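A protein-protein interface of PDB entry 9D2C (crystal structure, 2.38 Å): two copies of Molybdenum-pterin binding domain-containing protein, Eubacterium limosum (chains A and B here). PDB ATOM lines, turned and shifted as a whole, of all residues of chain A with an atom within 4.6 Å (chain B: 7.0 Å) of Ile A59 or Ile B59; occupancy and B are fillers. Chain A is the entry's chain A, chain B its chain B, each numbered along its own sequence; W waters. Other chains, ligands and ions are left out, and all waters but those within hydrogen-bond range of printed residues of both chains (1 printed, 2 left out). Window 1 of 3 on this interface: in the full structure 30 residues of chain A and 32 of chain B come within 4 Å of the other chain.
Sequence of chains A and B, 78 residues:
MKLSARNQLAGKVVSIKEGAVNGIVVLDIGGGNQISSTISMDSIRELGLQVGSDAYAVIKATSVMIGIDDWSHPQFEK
Of the 18 printed residues of chain B, 7 touch a printed residue of chain A.
Printed residues of chain A that touch a printed residue of chain B: Arg A6, Asn A7, Ala A57, Val A58, Ile A59, Ala A61, Ser A63 and Val A64.
Hydrophobic or aromatic side chains of chain A that line the printed part of chain B: Val A58, Ile A59, Ala A61 and Val A64.
ND2 of Asn A7 is in hydrogen-bond range of O of Ile A59, at 2.8 Å.
The backbone carbonyl oxygen (O) of Ile B59 lies within hydrogen-bond range of the side-chain amide nitrogen (ND2) of Asn B7 (2.9 Å).
CB of Arg A6 touches CB of Ser B36 (3.5 Å).
OD1 of Asn A7 touches CA of Ile B35, 3.1 Å away.
CA of Ala A57 touches O of Met B65 (3.6 Å).
Ile A59 touches Ile B59 (CD1 to CD1, 3.9 Å).
O of Ser B36 touches CA of Ala A61, 3.6 Å away.
Ser A63 touches Ser B63 (CB to CB, 3.7 Å).
CG1 of Val A64 touches CG2 of Ile B35, at 3.8 Å.
O of Ser B36 touches CG2 of Val A64 (3.5 Å).
Val A64 touches Val B58.
CG2 of Val A64 touches CG1 of Ile B59, at 3.8 Å.
The backbone NH of Ser B36 is in hydrogen-bond range of the side-chain amide oxygen of Asn A7.
The backbone NH (N) of Val A58 lies within hydrogen-bond range of the backbone carbonyl oxygen (O) of Met B65.
Val A58 touches Val B64, and with the chains exchanged Val A64 touches Val B58.
Ile B59 touches its own counterpart, Ile A59.
Ile A59 touches Val B64, and with the chains exchanged Val A64 touches Ile B59.
Ser B63 touches its own counterpart, Ser A63.
Water W1 lies within hydrogen-bond range of the side-chain hydroxyl of Ser A63 (2.4 Å), the backbone carbonyl oxygen of Ser B63 (2.8 Å) and the backbone NH of Lys A60 (3.2 Å).
Of the printed residues of chain B, Val A58 touches Val B64 (3.8 Å) and Met B65 (2.8 Å).
Of chain B, only Ile B59 and Val B64 come within 4 Å of Ile A59.
Lys A60 touches none of the printed residues of chain B.
Of the printed residues of chain B, Ser A63 touches Ser B63 (3.7 Å).
Of the printed residues of chain B, Val A64 touches Ile B35, Ser B36, Val B58 and Ile B59.
Of chain A, only Ile A59 and Val A64 come within 4 Å of Ile B59.
Printed residues of chain A within 4 Å of Val B64: Val A58 (3.8 Å) and Ile A59 (3.9 Å).
Printed residues of chain A within 4 Å of Met B65: Ala A57 and Val A58.
The nearest residue of chain A that does not touch Ile B59 is Ser A63 (4.3 Å).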
ATOM      1  N   ALA A   5     -18.135   5.252  29.670  1.00  0.00           N
ATOM      2  CA  ALA A   5     -16.720   5.120  29.353  1.00  0.00           C
ATOM      3  C   ALA A   5     -16.260   6.361  28.601  1.00  0.00           C
ATOM      4  O   ALA A   5     -16.867   6.747  27.594  1.00  0.00           O
ATOM      5  CB  ALA A   5     -16.477   3.863  28.517  1.00  0.00           C
ATOM      6  N   ARG A   6     -15.226   7.034  29.136  1.00  0.00           N
ATOM      7  CA  ARG A   6     -14.736   8.256  28.497  1.00  0.00           C
ATOM      8  C   ARG A   6     -14.062   7.971  27.164  1.00  0.00           C
ATOM      9  O   ARG A   6     -13.993   8.871  26.321  1.00  0.00           O
ATOM     10  CB  ARG A   6     -13.736   8.993  29.389  1.00  0.00           C
ATOM     11  CG  ARG A   6     -14.355   9.506  30.664  1.00  0.00           C
ATOM     12  CD  ARG A   6     -15.458  10.515  30.403  1.00  0.00           C
ATOM     13  NE  ARG A   6     -14.890  11.741  29.854  1.00  0.00           N
ATOM     14  CZ  ARG A   6     -15.584  12.725  29.294  1.00  0.00           C
ATOM     15  NH1 ARG A   6     -16.911  12.676  29.181  1.00  0.00           N
ATOM     16  NH2 ARG A   6     -14.930  13.790  28.836  1.00  0.00           N
ATOM     17  N   ASN A   7     -13.621   6.736  26.923  1.00  0.00           N
ATOM     18  CA  ASN A   7     -12.855   6.409  25.729  1.00  0.00           C
ATOM     19  C   ASN A   7     -13.664   5.452  24.862  1.00  0.00           C
ATOM     20  O   ASN A   7     -13.868   4.295  25.239  1.00  0.00           O
ATOM     21  CB  ASN A   7     -11.523   5.804  26.154  1.00  0.00           C
ATOM     22  CG  ASN A   7     -10.812   6.650  27.212  1.00  0.00           C
ATOM     23  OD1 ASN A   7     -10.277   7.714  26.912  1.00  0.00           O
ATOM     24  ND2 ASN A   7     -10.831   6.188  28.462  1.00  0.00           N
ATOM     25  N   ALA A  57     -12.984   0.522  20.306  1.00  0.00           N
ATOM     26  CA  ALA A  57     -12.292   0.187  21.546  1.00  0.00           C
ATOM     27  C   ALA A  57     -12.922   1.041  22.645  1.00  0.00           C
ATOM     28  O   ALA A  57     -12.927   2.276  22.548  1.00  0.00           O
ATOM     29  CB  ALA A  57     -10.795   0.448  21.437  1.00  0.00           C
ATOM     30  N   VAL A  58     -13.492   0.395  23.659  1.00  0.00           N
ATOM     31  CA  VAL A  58     -14.227   1.083  24.712  1.00  0.00           C
ATOM     32  C   VAL A  58     -13.492   0.850  26.022  1.00  0.00           C
ATOM     33  O   VAL A  58     -13.305  -0.301  26.443  1.00  0.00           O
ATOM     34  CB  VAL A  58     -15.682   0.609  24.791  1.00  0.00           C
ATOM     35  CG1 VAL A  58     -16.441   1.452  25.779  1.00  0.00           C
ATOM     36  CG2 VAL A  58     -16.319   0.708  23.435  1.00  0.00           C
ATOM     37  N   ILE A  59     -13.091   1.950  26.662  1.00  0.00           N
ATOM     38  CA  ILE A  59     -12.201   1.956  27.818  1.00  0.00           C
ATOM     39  C   ILE A  59     -12.677   2.999  28.819  1.00  0.00           C
ATOM     40  O   ILE A  59     -12.854   4.181  28.473  1.00  0.00           O
ATOM     41  CB  ILE A  59     -10.737   2.272  27.437  1.00  0.00           C
ATOM     42  CG1 ILE A  59     -10.236   1.366  26.307  1.00  0.00           C
ATOM     43  CG2 ILE A  59      -9.862   2.152  28.657  1.00  0.00           C
ATOM     44  CD1 ILE A  59      -9.266   2.052  25.380  1.00  0.00           C
ATOM     45  N   LYS A  60     -12.874   2.552  30.057  1.00  0.00           N
ATOM     46  CA  LYS A  60     -13.171   3.425  31.180  1.00  0.00           C
ATOM     47  C   LYS A  60     -11.955   4.268  31.536  1.00  0.00           C
ATOM     48  O   LYS A  60     -10.829   3.770  31.559  1.00  0.00           O
ATOM     49  CB  LYS A  60     -13.579   2.559  32.376  1.00  0.00           C
ATOM     50  CG  LYS A  60     -14.330   3.272  33.463  1.00  0.00           C
ATOM     51  CD  LYS A  60     -14.705   2.313  34.564  1.00  0.00           C
ATOM     52  CE  LYS A  60     -15.577   3.018  35.579  1.00  0.00           C
ATOM     53  NZ  LYS A  60     -14.879   4.180  36.187  1.00  0.00           N
ATOM     54  N   ALA A  61     -12.186   5.539  31.870  1.00  0.00           N
ATOM     55  CA  ALA A  61     -11.067   6.431  32.181  1.00  0.00           C
ATOM     56  C   ALA A  61     -10.233   5.920  33.353  1.00  0.00           C
ATOM     57  O   ALA A  61      -9.022   6.162  33.403  1.00  0.00           O
ATOM     58  CB  ALA A  61     -11.583   7.838  32.474  1.00  0.00           C
ATOM     59  N   SER A  63      -9.353   3.054  33.957  1.00  0.00           N
ATOM     60  CA  SER A  63      -8.462   1.990  33.521  1.00  0.00           C
ATOM     61  C   SER A  63      -7.216   2.507  32.820  1.00  0.00           C
ATOM     62  O   SER A  63      -6.324   1.700  32.530  1.00  0.00           O
ATOM     63  CB  SER A  63      -9.153   1.044  32.530  1.00  0.00           C
ATOM     64  OG  SER A  63     -10.254   0.384  33.100  1.00  0.00           O
ATOM     65  N   VAL A  64      -7.129   3.815  32.563  1.00  0.00           N
ATOM     66  CA  VAL A  64      -6.065   4.413  31.758  1.00  0.00           C
ATOM     67  C   VAL A  64      -5.042   5.084  32.660  1.00  0.00           C
ATOM     68  O   VAL A  64      -5.374   6.002  33.417  1.00  0.00           O
ATOM     69  CB  VAL A  64      -6.630   5.435  30.760  1.00  0.00           C
ATOM     70  CG1 VAL A  64      -5.514   6.007  29.895  1.00  0.00           C
ATOM     71  CG2 VAL A  64      -7.692   4.803  29.914  1.00  0.00           C
ATOM     72  N   LEU B   3       6.661  -2.414  29.767  1.00  0.00           N
ATOM     73  CA  LEU B   3       5.453  -2.909  30.403  1.00  0.00           C
ATOM     74  C   LEU B   3       4.693  -3.870  29.500  1.00  0.00           C
ATOM     75  O   LEU B   3       4.657  -3.714  28.273  1.00  0.00           O
ATOM     76  CB  LEU B   3       4.559  -1.736  30.802  1.00  0.00           C
ATOM     77  CG  LEU B   3       3.634  -1.940  31.998  1.00  0.00           C
ATOM     78  CD1 LEU B   3       4.513  -1.927  33.239  1.00  0.00           C
ATOM     79  CD2 LEU B   3       2.551  -0.846  32.038  1.00  0.00           C
ATOM     80  N   SER B   4       4.019  -4.827  30.151  1.00  0.00           N
ATOM     81  CA  SER B   4       3.221  -5.816  29.437  1.00  0.00           C
ATOM     82  C   SER B   4       1.950  -5.216  28.860  1.00  0.00           C
ATOM     83  O   SER B   4       1.288  -5.881  28.049  1.00  0.00           O
ATOM     84  CB  SER B   4       2.859  -6.991  30.354  1.00  0.00           C
ATOM     85  OG  SER B   4       2.032  -6.608  31.441  1.00  0.00           O
ATOM     86  N   ALA B   5       1.556  -4.018  29.306  1.00  0.00           N
ATOM     87  CA  ALA B   5       0.356  -3.372  28.781  1.00  0.00           C
ATOM     88  C   ALA B   5       0.403  -3.331  27.262  1.00  0.00           C
ATOM     89  O   ALA B   5       1.330  -2.777  26.672  1.00  0.00           O
ATOM     90  CB  ALA B   5       0.226  -1.960  29.353  1.00  0.00           C
ATOM     91  N   ARG B   6      -0.588  -3.928  26.615  1.00  0.00           N
ATOM     92  CA  ARG B   6      -0.519  -4.001  25.165  1.00  0.00           C
ATOM     93  C   ARG B   6      -0.725  -2.651  24.503  1.00  0.00           C
ATOM     94  O   ARG B   6      -0.422  -2.512  23.318  1.00  0.00           O
ATOM     95  CB  ARG B   6      -1.558  -4.964  24.604  1.00  0.00           C
ATOM     96  CG  ARG B   6      -1.410  -6.394  25.048  1.00  0.00           C
ATOM     97  CD  ARG B   6      -0.053  -6.998  24.756  1.00  0.00           C
ATOM     98  NE  ARG B   6       0.267  -7.289  23.364  1.00  0.00           N
ATOM     99  CZ  ARG B   6       1.496  -7.584  22.955  1.00  0.00           C
ATOM    100  NH1 ARG B   6       2.514  -7.594  23.799  1.00  0.00           N
ATOM    101  NH2 ARG B   6       1.710  -7.879  21.672  1.00  0.00           N
ATOM    102  N   ASN B   7      -1.291  -1.673  25.201  1.00  0.00           N
ATOM    103  CA  ASN B   7      -1.610  -0.400  24.569  1.00  0.00           C
ATOM    104  C   ASN B   7      -0.799   0.706  25.224  1.00  0.00           C
ATOM    105  O   ASN B   7      -0.988   0.985  26.415  1.00  0.00           O
ATOM    106  CB  ASN B   7      -3.108  -0.132  24.675  1.00  0.00           C
ATOM    107  CG  ASN B   7      -3.944  -1.325  24.235  1.00  0.00           C
ATOM    108  OD1 ASN B   7      -4.061  -1.626  23.044  1.00  0.00           O
ATOM    109  ND2 ASN B   7      -4.497  -2.042  25.213  1.00  0.00           N
ATOM    110  N   GLN B   8       0.086   1.346  24.433  1.00  0.00           N
ATOM    111  CA  GLN B   8       0.977   2.429  24.885  1.00  0.00           C
ATOM    112  C   GLN B   8       0.976   3.504  23.796  1.00  0.00           C
ATOM    113  O   GLN B   8       1.762   3.468  22.851  1.00  0.00           O
ATOM    114  CB  GLN B   8       2.367   1.869  25.175  1.00  0.00           C
ATOM    115  CG  GLN B   8       2.323   0.915  26.376  1.00  0.00           C
ATOM    116  CD  GLN B   8       3.631   0.208  26.690  1.00  0.00           C
ATOM    117  OE1 GLN B   8       3.620  -0.957  27.105  1.00  0.00           O
ATOM    118  NE2 GLN B   8       4.757   0.911  26.536  1.00  0.00           N
ATOM    119  N   LEU B   9       0.103   4.490  23.946  1.00  0.00           N
ATOM    120  CA  LEU B   9      -0.249   5.381  22.844  1.00  0.00           C
ATOM    121  C   LEU B   9       0.294   6.775  23.114  1.00  0.00           C
ATOM    122  O   LEU B   9      -0.163   7.458  24.036  1.00  0.00           O
ATOM    123  CB  LEU B   9      -1.766   5.404  22.666  1.00  0.00           C
ATOM    124  CG  LEU B   9      -2.393   4.046  22.310  1.00  0.00           C
ATOM    125  CD1 LEU B   9      -3.910   4.139  22.303  1.00  0.00           C
ATOM    126  CD2 LEU B   9      -1.906   3.514  20.951  1.00  0.00           C
ATOM    127  N   ILE B  35      -7.851  10.328  24.445  1.00  0.00           N
ATOM    128  CA  ILE B  35      -7.974   9.329  25.503  1.00  0.00           C
ATOM    129  C   ILE B  35      -8.032  10.054  26.833  1.00  0.00           C
ATOM    130  O   ILE B  35      -7.198  10.923  27.107  1.00  0.00           O
ATOM    131  CB  ILE B  35      -6.826   8.304  25.467  1.00  0.00           C
ATOM    132  CG1 ILE B  35      -6.903   7.552  24.132  1.00  0.00           C
ATOM    133  CG2 ILE B  35      -6.919   7.368  26.686  1.00  0.00           C
ATOM    134  CD1 ILE B  35      -5.873   6.498  23.928  1.00  0.00           C
ATOM    135  N   SER B  36      -9.022   9.716  27.646  1.00  0.00           N
ATOM    136  CA  SER B  36      -9.174  10.256  28.986  1.00  0.00           C
ATOM    137  C   SER B  36      -8.644   9.265  30.012  1.00  0.00           C
ATOM    138  O   SER B  36      -8.843   8.056  29.868  1.00  0.00           O
ATOM    139  CB  SER B  36     -10.644  10.551  29.275  1.00  0.00           C
ATOM    140  OG  SER B  36     -11.132  11.523  28.373  1.00  0.00           O
ATOM    141  N   ALA B  57      -0.699   7.164  26.910  1.00  0.00           N
ATOM    142  CA  ALA B  57      -1.844   6.511  27.534  1.00  0.00           C
ATOM    143  C   ALA B  57      -1.564   5.016  27.560  1.00  0.00           C
ATOM    144  O   ALA B  57      -1.394   4.404  26.498  1.00  0.00           O
ATOM    145  CB  ALA B  57      -3.131   6.786  26.760  1.00  0.00           C
ATOM    146  N   VAL B  58      -1.545   4.427  28.755  1.00  0.00           N
ATOM    147  CA  VAL B  58      -1.159   3.032  28.953  1.00  0.00           C
ATOM    148  C   VAL B  58      -2.370   2.258  29.433  1.00  0.00           C
ATOM    149  O   VAL B  58      -3.030   2.653  30.402  1.00  0.00           O
ATOM    150  CB  VAL B  58       0.009   2.890  29.941  1.00  0.00           C
ATOM    151  CG1 VAL B  58       0.376   1.418  30.080  1.00  0.00           C
ATOM    152  CG2 VAL B  58       1.238   3.736  29.471  1.00  0.00           C
ATOM    153  N   ILE B  59      -2.711   1.205  28.703  1.00  0.00           N
ATOM    154  CA  ILE B  59      -3.932   0.454  28.956  1.00  0.00           C
ATOM    155  C   ILE B  59      -3.658  -1.027  28.749  1.00  0.00           C
ATOM    156  O   ILE B  59      -3.189  -1.442  27.675  1.00  0.00           O
ATOM    157  CB  ILE B  59      -5.090   0.916  28.056  1.00  0.00           C
ATOM    158  CG1 ILE B  59      -5.258   2.438  28.118  1.00  0.00           C
ATOM    159  CG2 ILE B  59      -6.345   0.228  28.491  1.00  0.00           C
ATOM    160  CD1 ILE B  59      -5.714   3.001  26.819  1.00  0.00           C
ATOM    161  N   LYS B  60      -3.956  -1.807  29.794  1.00  0.00           N
ATOM    162  CA  LYS B  60      -3.900  -3.260  29.762  1.00  0.00           C
ATOM    163  C   LYS B  60      -4.977  -3.786  28.839  1.00  0.00           C
ATOM    164  O   LYS B  60      -6.097  -3.265  28.812  1.00  0.00           O
ATOM    165  CB  LYS B  60      -4.132  -3.832  31.165  1.00  0.00           C
ATOM    166  CG  LYS B  60      -3.642  -5.266  31.376  1.00  0.00           C
ATOM    167  CD  LYS B  60      -3.876  -5.717  32.827  1.00  0.00           C
ATOM    168  CE  LYS B  60      -3.241  -7.094  33.105  1.00  0.00           C
ATOM    169  NZ  LYS B  60      -3.764  -8.198  32.237  1.00  0.00           N
ATOM    170  N   ALA B  61      -4.646  -4.844  28.098  1.00  0.00           N
ATOM    171  CA  ALA B  61      -5.599  -5.382  27.136  1.00  0.00           C
ATOM    172  C   ALA B  61      -6.887  -5.835  27.811  1.00  0.00           C
ATOM    173  O   ALA B  61      -7.969  -5.714  27.227  1.00  0.00           O
ATOM    174  CB  ALA B  61      -4.975  -6.542  26.377  1.00  0.00           C
ATOM    175  N   THR B  62      -6.795  -6.386  29.026  1.00  0.00           N
ATOM    176  CA  THR B  62      -7.981  -6.908  29.702  1.00  0.00           C
ATOM    177  C   THR B  62      -8.932  -5.813  30.170  1.00  0.00           C
ATOM    178  O   THR B  62     -10.031  -6.128  30.641  1.00  0.00           O
ATOM    179  CB  THR B  62      -7.581  -7.789  30.889  1.00  0.00           C
ATOM    180  OG1 THR B  62      -6.523  -7.179  31.637  1.00  0.00           O
ATOM    181  CG2 THR B  62      -7.112  -9.143  30.414  1.00  0.00           C
ATOM    182  N   SER B  63      -8.529  -4.553  30.074  1.00  0.00           N
ATOM    183  CA  SER B  63      -9.371  -3.412  30.394  1.00  0.00           C
ATOM    184  C   SER B  63     -10.081  -2.850  29.164  1.00  0.00           C
ATOM    185  O   SER B  63     -10.806  -1.858  29.283  1.00  0.00           O
ATOM    186  CB  SER B  63      -8.532  -2.303  31.050  1.00  0.00           C
ATOM    187  OG  SER B  63      -7.936  -2.732  32.263  1.00  0.00           O
ATOM    188  N   VAL B  64      -9.846  -3.411  27.981  1.00  0.00           N
ATOM    189  CA  VAL B  64     -10.409  -2.871  26.750  1.00  0.00           C
ATOM    190  C   VAL B  64     -11.591  -3.721  26.321  1.00  0.00           C
ATOM    191  O   VAL B  64     -11.443  -4.914  26.061  1.00  0.00           O
ATOM    192  CB  VAL B  64      -9.373  -2.811  25.621  1.00  0.00           C
ATOM    193  CG1 VAL B  64     -10.035  -2.247  24.379  1.00  0.00           C
ATOM    194  CG2 VAL B  64      -8.203  -1.942  26.000  1.00  0.00           C
ATOM    195  N   MET B  65     -12.750  -3.098  26.191  1.00  0.00           N
ATOM    196  CA  MET B  65     -13.930  -3.738  25.629  1.00  0.00           C
ATOM    197  C   MET B  65     -14.089  -3.345  24.169  1.00  0.00           C
ATOM    198  O   MET B  65     -13.437  -2.419  23.676  1.00  0.00           O
ATOM    199  CB  MET B  65     -15.170  -3.352  26.427  1.00  0.00           C
ATOM    200  CG  MET B  65     -15.202  -3.954  27.815  1.00  0.00           C
ATOM    201  SD  MET B  65     -16.256  -2.987  28.919  1.00  0.00           S
ATOM    202  CE  MET B  65     -15.349  -1.441  29.061  1.00  0.00           C
HETATM  203  O   HOH W   1     -11.760  -0.215  31.309  1.00  0.00           O
